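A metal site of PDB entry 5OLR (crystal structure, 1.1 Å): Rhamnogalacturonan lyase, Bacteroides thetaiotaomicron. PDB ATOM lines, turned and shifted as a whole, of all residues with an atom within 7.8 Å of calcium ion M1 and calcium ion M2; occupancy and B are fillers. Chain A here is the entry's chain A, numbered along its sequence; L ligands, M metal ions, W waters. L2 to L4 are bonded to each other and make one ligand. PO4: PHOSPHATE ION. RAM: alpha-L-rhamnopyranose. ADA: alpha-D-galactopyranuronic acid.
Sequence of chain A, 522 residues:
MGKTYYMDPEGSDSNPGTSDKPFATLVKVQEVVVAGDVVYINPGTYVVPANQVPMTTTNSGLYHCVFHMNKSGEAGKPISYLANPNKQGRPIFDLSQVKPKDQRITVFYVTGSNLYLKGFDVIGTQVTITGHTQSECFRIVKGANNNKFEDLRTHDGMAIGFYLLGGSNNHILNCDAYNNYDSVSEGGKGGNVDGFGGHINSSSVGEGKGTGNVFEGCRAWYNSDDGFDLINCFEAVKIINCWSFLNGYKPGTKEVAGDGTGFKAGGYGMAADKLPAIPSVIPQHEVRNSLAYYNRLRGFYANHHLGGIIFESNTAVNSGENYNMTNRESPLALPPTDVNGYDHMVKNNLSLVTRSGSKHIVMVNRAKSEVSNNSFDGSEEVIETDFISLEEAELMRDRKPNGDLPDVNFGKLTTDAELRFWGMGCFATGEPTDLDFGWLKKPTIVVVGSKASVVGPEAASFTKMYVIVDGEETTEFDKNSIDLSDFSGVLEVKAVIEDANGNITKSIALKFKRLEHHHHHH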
ATOM      1  N   ILE A 160     -25.418 -15.385  -7.766  1.00  0.00           N
ATOM      2  CA  ILE A 160     -24.708 -14.244  -7.235  1.00  0.00           C
ATOM      3  C   ILE A 160     -23.216 -14.512  -7.346  1.00  0.00           C
ATOM      4  O   ILE A 160     -22.779 -15.649  -7.140  1.00  0.00           O
ATOM      5  CB  ILE A 160     -25.088 -14.067  -5.736  1.00  0.00           C
ATOM      6  CG1 ILE A 160     -26.597 -13.815  -5.562  1.00  0.00           C
ATOM      7  CG2 ILE A 160     -24.277 -12.994  -5.083  1.00  0.00           C
ATOM      8  CD1 ILE A 160     -27.124 -14.261  -4.218  1.00  0.00           C
ATOM      9  N   GLY A 190     -35.412 -12.599 -11.683  1.00  0.00           N
ATOM     10  CA  GLY A 190     -33.984 -12.347 -11.475  1.00  0.00           C
ATOM     11  C   GLY A 190     -33.651 -11.385 -10.348  1.00  0.00           C
ATOM     12  O   GLY A 190     -32.548 -10.838 -10.280  1.00  0.00           O
ATOM     13  N   GLY A 191     -34.578 -11.181  -9.403  1.00  0.00           N
ATOM     14  CA  GLY A 191     -34.423 -10.174  -8.369  1.00  0.00           C
ATOM     15  C   GLY A 191     -33.497 -10.475  -7.231  1.00  0.00           C
ATOM     16  O   GLY A 191     -33.362  -9.617  -6.356  1.00  0.00           O
ATOM     17  N   ASN A 192     -32.839 -11.634  -7.214  1.00  0.00           N
ATOM     18  CA  ASN A 192     -31.882 -11.924  -6.156  1.00  0.00           C
ATOM     19  C   ASN A 192     -30.465 -12.086  -6.659  1.00  0.00           C
ATOM     20  O   ASN A 192     -29.598 -12.427  -5.877  1.00  0.00           O
ATOM     21  CB  ASN A 192     -32.308 -13.166  -5.368  1.00  0.00           C
ATOM     22  CG  ASN A 192     -33.665 -13.001  -4.722  1.00  0.00           C
ATOM     23  OD1 ASN A 192     -33.993 -11.943  -4.204  1.00  0.00           O
ATOM     24  ND2 ASN A 192     -34.486 -14.012  -4.827  1.00  0.00           N
ATOM     25  N   VAL A 193     -30.228 -11.834  -7.949  1.00  0.00           N
ATOM     26  CA  VAL A 193     -28.871 -12.030  -8.508  1.00  0.00           C
ATOM     27  C   VAL A 193     -28.110 -10.706  -8.600  1.00  0.00           C
ATOM     28  O   VAL A 193     -28.334  -9.924  -9.504  1.00  0.00           O
ATOM     29  CB  VAL A 193     -28.898 -12.751  -9.839  1.00  0.00           C
ATOM     30  CG1 VAL A 193     -27.466 -13.082 -10.282  1.00  0.00           C
ATOM     31  CG2 VAL A 193     -29.718 -14.009  -9.763  1.00  0.00           C
ATOM     32  N   ASP A 194     -27.199 -10.490  -7.643  1.00  0.00           N
ATOM     33  CA  ASP A 194     -26.298  -9.377  -7.642  1.00  0.00           C
ATOM     34  C   ASP A 194     -24.901  -9.862  -8.069  1.00  0.00           C
ATOM     35  O   ASP A 194     -24.572 -11.025  -7.876  1.00  0.00           O
ATOM     36  CB  ASP A 194     -26.184  -8.768  -6.228  1.00  0.00           C
ATOM     37  CG  ASP A 194     -27.464  -8.158  -5.699  1.00  0.00           C
ATOM     38  OD1 ASP A 194     -28.297  -7.689  -6.519  1.00  0.00           O
ATOM     39  OD2 ASP A 194     -27.623  -8.073  -4.479  1.00  0.00           O
ATOM     40  N   GLY A 195     -24.087  -8.947  -8.555  1.00  0.00           N
ATOM     41  CA  GLY A 195     -22.681  -9.257  -8.794  1.00  0.00           C
ATOM     42  C   GLY A 195     -21.963  -9.513  -7.478  1.00  0.00           C
ATOM     43  O   GLY A 195     -21.330 -10.572  -7.310  1.00  0.00           O
ATOM     44  N   PHE A 196     -22.063  -8.536  -6.564  1.00  0.00           N
ATOM     45  CA  PHE A 196     -21.330  -8.514  -5.313  1.00  0.00           C
ATOM     46  C   PHE A 196     -22.242  -8.099  -4.187  1.00  0.00           C
ATOM     47  O   PHE A 196     -22.900  -7.039  -4.279  1.00  0.00           O
ATOM     48  CB  PHE A 196     -20.189  -7.499  -5.419  1.00  0.00           C
ATOM     49  CG  PHE A 196     -19.206  -7.797  -6.544  1.00  0.00           C
ATOM     50  CD1 PHE A 196     -19.411  -7.319  -7.815  1.00  0.00           C
ATOM     51  CD2 PHE A 196     -18.071  -8.559  -6.305  1.00  0.00           C
ATOM     52  CE1 PHE A 196     -18.518  -7.617  -8.846  1.00  0.00           C
ATOM     53  CE2 PHE A 196     -17.176  -8.836  -7.324  1.00  0.00           C
ATOM     54  CZ  PHE A 196     -17.417  -8.376  -8.581  1.00  0.00           C
ATOM     55  N   GLY A 197     -22.311  -8.915  -3.154  1.00  0.00           N
ATOM     56  CA  GLY A 197     -23.180  -8.685  -2.009  1.00  0.00           C
ATOM     57  C   GLY A 197     -22.404  -8.662  -0.724  1.00  0.00           C
ATOM     58  O   GLY A 197     -21.688  -9.619  -0.393  1.00  0.00           O
ATOM     59  N   HIS A 199     -23.198  -8.446   3.167  1.00  0.00           N
ATOM     60  CA  HIS A 199     -24.355  -8.623   4.074  1.00  0.00           C
ATOM     61  C   HIS A 199     -23.892  -9.278   5.378  1.00  0.00           C
ATOM     62  O   HIS A 199     -24.443 -10.276   5.825  1.00  0.00           O
ATOM     63  CB  HIS A 199     -25.463  -9.451   3.398  1.00  0.00           C
ATOM     64  CG  HIS A 199     -25.734  -9.090   1.988  1.00  0.00           C
ATOM     65  ND1 HIS A 199     -26.327  -7.905   1.623  1.00  0.00           N
ATOM     66  CD2 HIS A 199     -25.527  -9.785   0.844  1.00  0.00           C
ATOM     67  CE1 HIS A 199     -26.465  -7.894   0.308  1.00  0.00           C
ATOM     68  NE2 HIS A 199     -25.990  -9.020  -0.193  1.00  0.00           N
ATOM     69  N   SER A 224     -28.782  -9.454 -13.026  1.00  0.00           N
ATOM     70  CA  SER A 224     -30.196  -9.172 -13.194  1.00  0.00           C
ATOM     71  C   SER A 224     -30.789  -8.274 -12.119  1.00  0.00           C
ATOM     72  O   SER A 224     -31.748  -7.569 -12.400  1.00  0.00           O
ATOM     73  CB  SER A 224     -30.984 -10.463 -13.384  1.00  0.00           C
ATOM     74  OG  SER A 224     -30.807 -11.403 -12.325  1.00  0.00           O
ATOM     75  N   ASP A 225     -30.204  -8.255 -10.917  1.00  0.00           N
ATOM     76  CA  ASP A 225     -30.680  -7.375  -9.884  1.00  0.00           C
ATOM     77  C   ASP A 225     -29.784  -6.151  -9.806  1.00  0.00           C
ATOM     78  O   ASP A 225     -29.973  -5.202 -10.592  1.00  0.00           O
ATOM     79  CB  ASP A 225     -30.893  -8.153  -8.547  1.00  0.00           C
ATOM     80  CG  ASP A 225     -31.796  -7.465  -7.567  1.00  0.00           C
ATOM     81  OD1 ASP A 225     -32.921  -7.054  -7.987  1.00  0.00           O
ATOM     82  OD2 ASP A 225     -31.471  -7.370  -6.379  1.00  0.00           O
ATOM     83  N   ASP A 226     -28.812  -6.133  -8.864  1.00  0.00           N
ATOM     84  CA  ASP A 226     -27.898  -4.989  -8.667  1.00  0.00           C
ATOM     85  C   ASP A 226     -26.468  -5.374  -8.999  1.00  0.00           C
ATOM     86  O   ASP A 226     -26.099  -6.549  -8.907  1.00  0.00           O
ATOM     87  CB  ASP A 226     -27.994  -4.527  -7.215  1.00  0.00           C
ATOM     88  CG  ASP A 226     -29.408  -4.210  -6.784  1.00  0.00           C
ATOM     89  OD1 ASP A 226     -30.093  -3.406  -7.468  1.00  0.00           O
ATOM     90  OD2 ASP A 226     -29.843  -4.750  -5.739  1.00  0.00           O
ATOM     91  N   GLY A 227     -25.637  -4.387  -9.287  1.00  0.00           N
ATOM     92  CA  GLY A 227     -24.227  -4.689  -9.401  1.00  0.00           C
ATOM     93  C   GLY A 227     -23.587  -5.019  -8.053  1.00  0.00           C
ATOM     94  O   GLY A 227     -22.957  -6.070  -7.891  1.00  0.00           O
ATOM     95  N   PHE A 228     -23.759  -4.107  -7.099  1.00  0.00           N
ATOM     96  CA  PHE A 228     -23.208  -4.201  -5.739  1.00  0.00           C
ATOM     97  C   PHE A 228     -24.369  -3.879  -4.778  1.00  0.00           C
ATOM     98  O   PHE A 228     -25.126  -2.935  -5.008  1.00  0.00           O
ATOM     99  CB  PHE A 228     -22.097  -3.169  -5.489  1.00  0.00           C
ATOM    100  CG  PHE A 228     -20.859  -3.399  -6.317  1.00  0.00           C
ATOM    101  CD1 PHE A 228     -20.823  -3.024  -7.643  1.00  0.00           C
ATOM    102  CD2 PHE A 228     -19.744  -4.002  -5.783  1.00  0.00           C
ATOM    103  CE1 PHE A 228     -19.673  -3.254  -8.436  1.00  0.00           C
ATOM    104  CE2 PHE A 228     -18.612  -4.217  -6.541  1.00  0.00           C
ATOM    105  CZ  PHE A 228     -18.598  -3.870  -7.858  1.00  0.00           C
ATOM    106  N   ASP A 229     -24.470  -4.651  -3.695  1.00  0.00           N
ATOM    107  CA  ASP A 229     -25.573  -4.519  -2.733  1.00  0.00           C
ATOM    108  C   ASP A 229     -25.058  -4.789  -1.333  1.00  0.00           C
ATOM    109  O   ASP A 229     -24.524  -5.876  -1.070  1.00  0.00           O
ATOM    110  CB  ASP A 229     -26.689  -5.473  -3.190  1.00  0.00           C
ATOM    111  CG  ASP A 229     -27.903  -5.514  -2.291  1.00  0.00           C
ATOM    112  OD1 ASP A 229     -27.802  -5.297  -1.086  1.00  0.00           O
ATOM    113  OD2 ASP A 229     -28.993  -5.877  -2.841  1.00  0.00           O
ATOM    114  N   LEU A 230     -25.249  -3.799  -0.461  1.00  0.00           N
ATOM    115  CA  LEU A 230     -24.814  -3.826   0.938  1.00  0.00           C
ATOM    116  C   LEU A 230     -26.006  -3.794   1.897  1.00  0.00           C
ATOM    117  O   LEU A 230     -25.860  -3.342   3.031  1.00  0.00           O
ATOM    118  CB  LEU A 230     -23.889  -2.638   1.254  1.00  0.00           C
ATOM    119  CG  LEU A 230     -22.660  -2.479   0.352  1.00  0.00           C
ATOM    120  CD1 LEU A 230     -21.816  -1.315   0.835  1.00  0.00           C
ATOM    121  CD2 LEU A 230     -21.812  -3.749   0.293  1.00  0.00           C
ATOM    122  N   ILE A 231     -27.172  -4.321   1.510  1.00  0.00           N
ATOM    123  CA  ILE A 231     -28.294  -4.353   2.463  1.00  0.00           C
ATOM    124  C   ILE A 231     -27.981  -5.290   3.637  1.00  0.00           C
ATOM    125  O   ILE A 231     -27.258  -6.258   3.521  1.00  0.00           O
ATOM    126  CB  ILE A 231     -29.619  -4.789   1.752  1.00  0.00           C
ATOM    127  CG1 ILE A 231     -30.843  -4.250   2.486  1.00  0.00           C
ATOM    128  CG2 ILE A 231     -29.680  -6.286   1.535  1.00  0.00           C
ATOM    129  CD1 ILE A 231     -32.160  -4.551   1.784  1.00  0.00           C
ATOM    130  N   GLY A 258     -34.460  -7.319 -12.593  1.00  0.00           N
ATOM    131  CA  GLY A 258     -34.554  -6.883 -11.220  1.00  0.00           C
ATOM    132  C   GLY A 258     -34.341  -5.411 -10.998  1.00  0.00           C
ATOM    133  O   GLY A 258     -34.605  -4.591 -11.839  1.00  0.00           O
ATOM    134  N   ASP A 259     -33.810  -5.106  -9.824  1.00  0.00           N
ATOM    135  CA  ASP A 259     -33.867  -3.767  -9.272  1.00  0.00           C
ATOM    136  C   ASP A 259     -32.998  -2.733  -9.995  1.00  0.00           C
ATOM    137  O   ASP A 259     -33.313  -1.541  -9.978  1.00  0.00           O
ATOM    138  CB  ASP A 259     -33.489  -3.819  -7.780  1.00  0.00           C
ATOM    139  CG  ASP A 259     -34.483  -4.591  -6.905  1.00  0.00           C
ATOM    140  OD1 ASP A 259     -35.676  -4.617  -7.257  1.00  0.00           O
ATOM    141  OD2 ASP A 259     -34.105  -5.183  -5.820  1.00  0.00           O
ATOM    142  N   GLY A 260     -31.876  -3.143 -10.603  1.00  0.00           N
ATOM    143  CA  GLY A 260     -31.106  -2.227 -11.429  1.00  0.00           C
ATOM    144  C   GLY A 260     -30.452  -1.069 -10.722  1.00  0.00           C
ATOM    145  O   GLY A 260     -30.487   0.063 -11.242  1.00  0.00           O
ATOM    146  N   THR A 261     -29.797  -1.367  -9.586  1.00  0.00           N
ATOM    147  CA  THR A 261     -28.962  -0.377  -8.940  1.00  0.00           C
ATOM    148  C   THR A 261     -27.518  -0.642  -9.288  1.00  0.00           C
ATOM    149  O   THR A 261     -27.069  -1.796  -9.233  1.00  0.00           O
ATOM    150  CB  THR A 261     -29.073  -0.430  -7.400  1.00  0.00           C
ATOM    151  OG1 THR A 261     -30.376  -0.793  -7.001  1.00  0.00           O
ATOM    152  CG2 THR A 261     -28.648   0.865  -6.746  1.00  0.00           C
ATOM    153  N   LYS A 264     -26.032  -0.295  -4.425  1.00  0.00           N
ATOM    154  CA  LYS A 264     -27.073  -0.266  -3.390  1.00  0.00           C
ATOM    155  C   LYS A 264     -26.286  -0.349  -2.080  1.00  0.00           C
ATOM    156  O   LYS A 264     -25.836  -1.399  -1.708  1.00  0.00           O
ATOM    157  CB  LYS A 264     -28.038  -1.440  -3.619  1.00  0.00           C
ATOM    158  CG  LYS A 264     -29.113  -1.566  -2.567  1.00  0.00           C
ATOM    159  CD  LYS A 264     -30.133  -2.625  -2.954  1.00  0.00           C
ATOM    160  CE  LYS A 264     -31.160  -2.120  -3.949  1.00  0.00           C
ATOM    161  NZ  LYS A 264     -31.945  -3.262  -4.511  1.00  0.00           N
ATOM    162  N   ASN A 303     -30.424   3.472  -0.241  1.00  0.00           N
ATOM    163  CA  ASN A 303     -31.274   2.327  -0.012  1.00  0.00           C
ATOM    164  C   ASN A 303     -31.896   2.287   1.378  1.00  0.00           C
ATOM    165  O   ASN A 303     -31.980   1.225   1.981  1.00  0.00           O
ATOM    166  CB  ASN A 303     -30.522   1.016  -0.308  1.00  0.00           C
ATOM    167  CG  ASN A 303     -31.455  -0.168  -0.418  1.00  0.00           C
ATOM    168  OD1 ASN A 303     -32.482  -0.051  -1.061  1.00  0.00           O
ATOM    169  ND2 ASN A 303     -31.110  -1.295   0.190  1.00  0.00           N
HETATM  170  P   PO4 L   1     -32.400  -6.069  -2.260  1.00  0.00           P
HETATM  171  O1  PO4 L   1     -33.053  -4.681  -2.390  1.00  0.00           O
HETATM  172  O2  PO4 L   1     -33.390  -6.967  -1.561  1.00  0.00           O
HETATM  173  O3  PO4 L   1     -31.167  -5.919  -1.371  1.00  0.00           O
HETATM  174  O4  PO4 L   1     -32.003  -6.529  -3.624  1.00  0.00           O
HETATM  175  C1  RAM L   2     -32.888  -9.943   0.421  1.00  0.00           C
HETATM  176  C2  RAM L   2     -33.029 -11.454   0.541  1.00  0.00           C
HETATM  177  C3  RAM L   2     -32.150 -12.158  -0.507  1.00  0.00           C
HETATM  178  C4  RAM L   2     -30.708 -11.701  -0.360  1.00  0.00           C
HETATM  179  C5  RAM L   2     -30.669 -10.177  -0.514  1.00  0.00           C
HETATM  180  C6  RAM L   2     -29.283  -9.590  -0.324  1.00  0.00           C
HETATM  181  O1  RAM L   2     -33.461  -9.496  -0.787  1.00  0.00           O
HETATM  182  O2  RAM L   2     -32.535 -11.770   1.844  1.00  0.00           O
HETATM  183  O3  RAM L   2     -32.308 -13.577  -0.371  1.00  0.00           O
HETATM  184  O4  RAM L   2     -29.918 -12.271  -1.399  1.00  0.00           O
HETATM  185  O5  RAM L   2     -31.495  -9.596   0.486  1.00  0.00           O
HETATM  186  C1  ADA L   3     -33.370 -12.509   2.731  1.00  0.00           C
HETATM  187  C2  ADA L   3     -32.902 -12.253   4.160  1.00  0.00           C
HETATM  188  C3  ADA L   3     -31.564 -12.901   4.391  1.00  0.00           C
HETATM  189  C4  ADA L   3     -31.612 -14.364   3.983  1.00  0.00           C
HETATM  190  C5  ADA L   3     -32.068 -14.491   2.534  1.00  0.00           C
HETATM  191  C6  ADA L   3     -32.104 -15.899   2.030  1.00  0.00           C
HETATM  192  O2  ADA L   3     -32.795 -10.840   4.376  1.00  0.00           O
HETATM  193  O3  ADA L   3     -31.186 -12.736   5.752  1.00  0.00           O
HETATM  194  O4  ADA L   3     -32.505 -15.116   4.828  1.00  0.00           O
HETATM  195  O5  ADA L   3     -33.382 -13.907   2.403  1.00  0.00           O
HETATM  196  O6B ADA L   3     -30.995 -16.497   1.976  1.00  0.00           O
HETATM  197  O6A ADA L   3     -33.201 -16.411   1.664  1.00  0.00           O
HETATM  198  C1  RAM L   4     -31.894 -15.773   5.902  1.00  0.00           C
HETATM  199  C2  RAM L   4     -32.923 -16.084   6.950  1.00  0.00           C
HETATM  200  C3  RAM L   4     -33.810 -17.189   6.389  1.00  0.00           C
HETATM  201  C4  RAM L   4     -32.972 -18.378   5.898  1.00  0.00           C
HETATM  202  C5  RAM L   4     -31.908 -17.919   4.884  1.00  0.00           C
HETATM  203  C6  RAM L   4     -30.972 -19.038   4.461  1.00  0.00           C
HETATM  204  O2  RAM L   4     -32.247 -16.540   8.119  1.00  0.00           O
HETATM  205  O3  RAM L   4     -34.736 -17.641   7.388  1.00  0.00           O
HETATM  206  O4  RAM L   4     -33.805 -19.322   5.263  1.00  0.00           O
HETATM  207  O5  RAM L   4     -31.145 -16.885   5.487  1.00  0.00           O
HETATM  208 CA    CA M   1     -33.544  -7.495  -5.293  1.00  0.00          CA
HETATM  209 CA    CA M   2     -29.873  -6.927  -4.737  1.00  0.00          CA
HETATM  210  O   HOH W   1     -35.785  -7.814  -6.386  1.00  0.00           O
HETATM  211  O   HOH W   2     -33.019  -9.520  -3.601  1.00  0.00           O
HETATM  212  O   HOH W   3     -30.328  -9.106  -4.020  1.00  0.00           O
HETATM  213  O   HOH W   4     -35.264  -7.350  -3.504  1.00  0.00           O
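Water W2 lies within hydrogen-bond range of OD1 of Asn 192 (2.7 Å) and O1 of RAM L2 (2.8 Å).
Four residues have an atom within 4 Å of calcium ion M2: Asp 194, Asp 225, Asp 226 and Asp 229.
N of Asp 225 is in hydrogen-bond range of O of Val 193 (2.9 Å). O of Asp 225 lies within hydrogen-bond range of N of Gly 260 (2.8 Å). The side-chain carboxylate of Asp 229 sits at hydrogen-bond distance from the backbone NH of Ile 231 (2.8 Å). The backbone NH (N) of Asp 229 sits at hydrogen-bond distance from the backbone carbonyl oxygen (O) of Phe 196 (2.9 Å). The side-chain carboxylate (OD1) of Asp 226 is in salt-bridge range of the side-chain amino group (NZ) of Lys 264 (3.5 Å). The side-chain carboxylate (OD1) of Asp 226 sits at hydrogen-bond distance from the side-chain hydroxyl (OG1) of Thr 261 (2.7 Å). O of Asp 226 is in hydrogen-bond range of N of Gly 195, at 3.1 Å. OD2 of Asp 259 sits close to NZ of Lys 264 (3.2 Å).
Three residues have an atom within 4 Å of calcium ion M1: Gly 191, Asp 225 and Asp 259.
Calcium ion M2 is bound by OD2 of Asp 225, 2.3 Å away. Calcium ion M2 is bound by water W3 (2.3 Å). OD2 of Asp 229 binds calcium ion M2 (2.3 Å). Calcium ion M2 is bound by OD2 of Asp 226, 2.4 Å away. Calcium ion M2 is bound by O4 of PO4 L1, 2.4 Å away. The side-chain carboxylate (OD1) of Asp 194 is bound to calcium ion M2 (2.5 Å). Calcium ion M2 is bound by OD2 of Asp 194, 2.5 Å away.
Calcium ion M1 is bound by the side-chain carboxylate (OD2) of Asp 225 (2.3 Å), the backbone carbonyl oxygen (O) of Gly 191 (2.4 Å), the side-chain carboxylate (OD2) of Asp 259 (2.4 Å), an oxygen (O4) of PO4 L1 (2.5 Å), water W4 (2.5 Å), water W1 (2.5 Å), water W2 (2.7 Å) and the side-chain carboxylate (OD1) of Asp 225 (2.8 Å).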
